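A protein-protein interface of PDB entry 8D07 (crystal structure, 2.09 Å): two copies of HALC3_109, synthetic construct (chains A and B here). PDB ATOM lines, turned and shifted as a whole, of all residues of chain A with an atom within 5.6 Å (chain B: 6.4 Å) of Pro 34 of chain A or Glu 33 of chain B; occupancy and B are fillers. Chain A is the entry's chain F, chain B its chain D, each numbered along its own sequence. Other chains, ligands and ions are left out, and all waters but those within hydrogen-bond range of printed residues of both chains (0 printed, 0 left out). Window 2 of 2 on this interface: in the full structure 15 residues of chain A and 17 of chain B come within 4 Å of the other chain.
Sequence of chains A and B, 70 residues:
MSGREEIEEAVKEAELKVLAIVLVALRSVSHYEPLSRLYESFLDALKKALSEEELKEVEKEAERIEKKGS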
ATOM      1  N   TYR A  32      31.433  -5.305 -11.108  1.00  0.00           N
ATOM      2  CA  TYR A  32      30.497  -4.350 -10.530  1.00  0.00           C
ATOM      3  C   TYR A  32      29.343  -4.165 -11.506  1.00  0.00           C
ATOM      4  O   TYR A  32      29.499  -3.512 -12.540  1.00  0.00           O
ATOM      5  CB  TYR A  32      31.157  -3.007 -10.232  1.00  0.00           C
ATOM      6  CG  TYR A  32      32.341  -3.102  -9.304  1.00  0.00           C
ATOM      7  CD1 TYR A  32      33.609  -3.367  -9.796  1.00  0.00           C
ATOM      8  CD2 TYR A  32      32.183  -2.971  -7.931  1.00  0.00           C
ATOM      9  CE1 TYR A  32      34.694  -3.457  -8.954  1.00  0.00           C
ATOM     10  CE2 TYR A  32      33.265  -3.071  -7.075  1.00  0.00           C
ATOM     11  CZ  TYR A  32      34.520  -3.312  -7.598  1.00  0.00           C
ATOM     12  OH  TYR A  32      35.614  -3.413  -6.767  1.00  0.00           O
ATOM     13  N   GLU A  33      28.186  -4.725 -11.175  1.00  0.00           N
ATOM     14  CA  GLU A  33      27.028  -4.584 -12.042  1.00  0.00           C
ATOM     15  C   GLU A  33      26.509  -3.152 -12.001  1.00  0.00           C
ATOM     16  O   GLU A  33      26.663  -2.457 -10.994  1.00  0.00           O
ATOM     17  CB  GLU A  33      25.926  -5.549 -11.617  1.00  0.00           C
ATOM     18  CG  GLU A  33      26.400  -6.969 -11.346  1.00  0.00           C
ATOM     19  CD  GLU A  33      26.529  -7.794 -12.608  1.00  0.00           C
ATOM     20  OE1 GLU A  33      25.713  -7.592 -13.537  1.00  0.00           O
ATOM     21  OE2 GLU A  33      27.443  -8.649 -12.665  1.00  0.00           O
ATOM     22  N   PRO A  34      25.897  -2.679 -13.090  1.00  0.00           N
ATOM     23  CA  PRO A  34      25.746  -3.358 -14.381  1.00  0.00           C
ATOM     24  C   PRO A  34      26.951  -3.204 -15.296  1.00  0.00           C
ATOM     25  O   PRO A  34      26.777  -3.353 -16.496  1.00  0.00           O
ATOM     26  CB  PRO A  34      24.509  -2.680 -14.978  1.00  0.00           C
ATOM     27  CG  PRO A  34      24.564  -1.280 -14.432  1.00  0.00           C
ATOM     28  CD  PRO A  34      25.115  -1.430 -13.032  1.00  0.00           C
ATOM     29  N   LEU A  35      28.161  -2.913 -14.809  1.00  0.00           N
ATOM     30  CA  LEU A  35      29.270  -2.707 -15.739  1.00  0.00           C
ATOM     31  C   LEU A  35      29.560  -3.963 -16.536  1.00  0.00           C
ATOM     32  O   LEU A  35      29.963  -3.868 -17.698  1.00  0.00           O
ATOM     33  CB  LEU A  35      30.535  -2.232 -15.016  1.00  0.00           C
ATOM     34  CG  LEU A  35      30.341  -0.918 -14.256  1.00  0.00           C
ATOM     35  CD1 LEU A  35      31.590  -0.512 -13.479  1.00  0.00           C
ATOM     36  CD2 LEU A  35      29.921   0.168 -15.223  1.00  0.00           C
ATOM     37  N   SER A  36      29.297  -5.148 -15.964  1.00  0.00           N
ATOM     38  CA  SER A  36      29.468  -6.368 -16.741  1.00  0.00           C
ATOM     39  C   SER A  36      28.636  -6.337 -18.017  1.00  0.00           C
ATOM     40  O   SER A  36      29.007  -6.966 -19.009  1.00  0.00           O
ATOM     41  CB  SER A  36      29.112  -7.610 -15.906  1.00  0.00           C
ATOM     42  OG  SER A  36      27.705  -7.767 -15.769  1.00  0.00           O
ATOM     43  N   ARG A  37      27.512  -5.625 -18.021  1.00  0.00           N
ATOM     44  CA  ARG A  37      26.764  -5.494 -19.269  1.00  0.00           C
ATOM     45  C   ARG A  37      27.520  -4.629 -20.281  1.00  0.00           C
ATOM     46  O   ARG A  37      27.573  -4.960 -21.473  1.00  0.00           O
ATOM     47  CB  ARG A  37      25.367  -4.930 -18.988  1.00  0.00           C
ATOM     48  CG  ARG A  37      24.465  -5.875 -18.113  1.00  0.00           C
ATOM     49  CD  ARG A  37      23.069  -5.250 -17.926  1.00  0.00           C
ATOM     50  NE  ARG A  37      22.116  -6.087 -17.192  1.00  0.00           N
ATOM     51  CZ  ARG A  37      21.308  -6.996 -17.728  1.00  0.00           C
ATOM     52  NH1 ARG A  37      21.362  -7.305 -19.017  1.00  0.00           N
ATOM     53  NH2 ARG A  37      20.417  -7.608 -16.948  1.00  0.00           N
ATOM     54  N   LEU A  38      28.145  -3.534 -19.828  1.00  0.00           N
ATOM     55  CA  LEU A  38      28.924  -2.734 -20.778  1.00  0.00           C
ATOM     56  C   LEU A  38      30.155  -3.506 -21.241  1.00  0.00           C
ATOM     57  O   LEU A  38      30.542  -3.419 -22.414  1.00  0.00           O
ATOM     58  CB  LEU A  38      29.314  -1.390 -20.154  1.00  0.00           C
ATOM     59  CG  LEU A  38      30.068  -0.340 -20.997  1.00  0.00           C
ATOM     60  CD1 LEU A  38      29.449  -0.143 -22.412  1.00  0.00           C
ATOM     61  CD2 LEU A  38      30.101   0.980 -20.223  1.00  0.00           C
ATOM     62  N   VAL B  29      23.438  -0.985 -23.972  1.00  0.00           N
ATOM     63  CA  VAL B  29      23.182  -1.132 -22.547  1.00  0.00           C
ATOM     64  C   VAL B  29      22.532   0.100 -21.963  1.00  0.00           C
ATOM     65  O   VAL B  29      22.465   0.227 -20.736  1.00  0.00           O
ATOM     66  CB  VAL B  29      24.472  -1.472 -21.786  1.00  0.00           C
ATOM     67  CG1 VAL B  29      24.998  -2.829 -22.235  1.00  0.00           C
ATOM     68  CG2 VAL B  29      25.522  -0.370 -22.014  1.00  0.00           C
ATOM     69  N   SER B  30      22.029   1.011 -22.815  1.00  0.00           N
ATOM     70  CA  SER B  30      21.655   2.365 -22.417  1.00  0.00           C
ATOM     71  C   SER B  30      20.387   2.427 -21.585  1.00  0.00           C
ATOM     72  O   SER B  30      20.009   3.522 -21.173  1.00  0.00           O
ATOM     73  CB  SER B  30      21.473   3.268 -23.651  1.00  0.00           C
ATOM     74  OG  SER B  30      20.253   2.979 -24.319  1.00  0.00           O
ATOM     75  N   HIS B  31      19.708   1.320 -21.333  1.00  0.00           N
ATOM     76  CA  HIS B  31      18.536   1.345 -20.480  1.00  0.00           C
ATOM     77  C   HIS B  31      18.770   0.674 -19.136  1.00  0.00           C
ATOM     78  O   HIS B  31      17.836   0.595 -18.331  1.00  0.00           O
ATOM     79  CB  HIS B  31      17.352   0.710 -21.215  1.00  0.00           C
ATOM     80  CG  HIS B  31      16.982   1.436 -22.475  1.00  0.00           C
ATOM     81  ND1 HIS B  31      16.930   0.815 -23.706  1.00  0.00           N
ATOM     82  CD2 HIS B  31      16.667   2.735 -22.697  1.00  0.00           C
ATOM     83  CE1 HIS B  31      16.591   1.697 -24.630  1.00  0.00           C
ATOM     84  NE2 HIS B  31      16.426   2.869 -24.045  1.00  0.00           N
ATOM     85  N   TYR B  32      19.989   0.208 -18.852  1.00  0.00           N
ATOM     86  CA  TYR B  32      20.310  -0.246 -17.505  1.00  0.00           C
ATOM     87  C   TYR B  32      20.888   0.914 -16.710  1.00  0.00           C
ATOM     88  O   TYR B  32      21.849   1.565 -17.146  1.00  0.00           O
ATOM     89  CB  TYR B  32      21.273  -1.439 -17.513  1.00  0.00           C
ATOM     90  CG  TYR B  32      20.718  -2.606 -18.274  1.00  0.00           C
ATOM     91  CD1 TYR B  32      19.880  -3.525 -17.664  1.00  0.00           C
ATOM     92  CD2 TYR B  32      20.996  -2.764 -19.618  1.00  0.00           C
ATOM     93  CE1 TYR B  32      19.351  -4.582 -18.375  1.00  0.00           C
ATOM     94  CE2 TYR B  32      20.481  -3.817 -20.331  1.00  0.00           C
ATOM     95  CZ  TYR B  32      19.664  -4.718 -19.709  1.00  0.00           C
ATOM     96  OH  TYR B  32      19.163  -5.748 -20.455  1.00  0.00           O
ATOM     97  N   GLU B  33      20.284   1.170 -15.558  1.00  0.00           N
ATOM     98  CA  GLU B  33      20.738   2.217 -14.659  1.00  0.00           C
ATOM     99  C   GLU B  33      22.085   1.837 -14.047  1.00  0.00           C
ATOM    100  O   GLU B  33      22.264   0.695 -13.622  1.00  0.00           O
ATOM    101  CB  GLU B  33      19.700   2.445 -13.551  1.00  0.00           C
ATOM    102  CG  GLU B  33      19.232   1.187 -12.742  1.00  0.00           C
ATOM    103  CD  GLU B  33      18.540   0.085 -13.568  1.00  0.00           C
ATOM    104  OE1 GLU B  33      17.654   0.412 -14.395  1.00  0.00           O
ATOM    105  OE2 GLU B  33      18.848  -1.110 -13.346  1.00  0.00           O
ATOM    106  N   PRO B  34      23.049   2.757 -13.986  1.00  0.00           N
ATOM    107  CA  PRO B  34      22.997   4.126 -14.513  1.00  0.00           C
ATOM    108  C   PRO B  34      23.687   4.269 -15.865  1.00  0.00           C
ATOM    109  O   PRO B  34      24.104   5.370 -16.212  1.00  0.00           O
ATOM    110  CB  PRO B  34      23.730   4.925 -13.433  1.00  0.00           C
ATOM    111  CG  PRO B  34      24.812   3.967 -12.960  1.00  0.00           C
ATOM    112  CD  PRO B  34      24.253   2.549 -13.158  1.00  0.00           C
ATOM    113  N   LEU B  35      23.816   3.205 -16.664  1.00  0.00           N
ATOM    114  CA  LEU B  35      24.535   3.335 -17.928  1.00  0.00           C
ATOM    115  C   LEU B  35      23.872   4.355 -18.853  1.00  0.00           C
ATOM    116  O   LEU B  35      24.551   4.964 -19.689  1.00  0.00           O
ATOM    117  CB  LEU B  35      24.677   1.961 -18.593  1.00  0.00           C
ATOM    118  CG  LEU B  35      25.248   0.929 -17.600  1.00  0.00           C
ATOM    119  CD1 LEU B  35      25.411  -0.460 -18.191  1.00  0.00           C
ATOM    120  CD2 LEU B  35      26.608   1.398 -17.057  1.00  0.00           C
ATOM    121  N   SER B  36      22.569   4.623 -18.671  1.00  0.00           N
ATOM    122  CA  SER B  36      21.917   5.643 -19.483  1.00  0.00           C
ATOM    123  C   SER B  36      22.537   7.014 -19.238  1.00  0.00           C
ATOM    124  O   SER B  36      22.572   7.855 -20.144  1.00  0.00           O
ATOM    125  CB  SER B  36      20.409   5.693 -19.206  1.00  0.00           C
ATOM    126  OG  SER B  36      20.060   6.679 -18.249  1.00  0.00           O
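Among the printed residues, merely in contact across the chains: Pro 34 of chain A with Glu 33 of chain B, Arg 37 of chain A with Val 29 of chain B, Pro 34 of chain A with Leu 35 of chain B, Leu 38 of chain A with Val 29 of chain B and Leu 35 of chain A with Leu 35 of chain B.
Pro 34 of chain A touches Glu 33 of chain B, but with the chains exchanged Glu 33 of chain A does not touch Pro 34 of chain B (6.0 Å).
Pro 34 of chain A touches Leu 35 of chain B, but with the chains exchanged Leu 35 of chain A does not touch Pro 34 of chain B (6.5 Å).
Leu 35 of chain B touches its own counterpart, Leu 35 of chain A.
Positions printed for both chains: 32, 33, 34, 35 and 36.
Of the 7 printed residues of chain A, 4 touch a printed residue of chain B.
Printed residues of chain A that touch a printed residue of chain B: Pro 34, Leu 35, Arg 37 and Leu 38.
Along chain A the printed residues that touch a printed residue of chain B span positions 34 to 38.
Among the printed residues, 6 pairs touch across the chains.
Glu 33 of chain B touches one residue of chain A.
Printed residues of chain B within 4 Å of Leu 35 of chain A: Leu 35.
Of the printed residues of chain A, Leu 35 of chain B touches Pro 34 (3.6 Å) and Leu 35 (3.98 Å).
Of the printed residues of chain A, Tyr 32 of chain B touches Arg 37 (3.1 Å).
Printed residues of chain B within 4 Å of Leu 38 of chain A: Val 29.
The nearest printed residue of chain A that does not touch Glu 33 of chain B is Glu 33 of chain A (6.0 Å).
The nearest printed residue of chain A that does not touch Val 29 of chain B is Pro 34 of chain A (6.0 Å).
OH of Tyr 32 of chain B sits at hydrogen-bond distance from NH1 of Arg 37 of chain A (3.1 Å).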
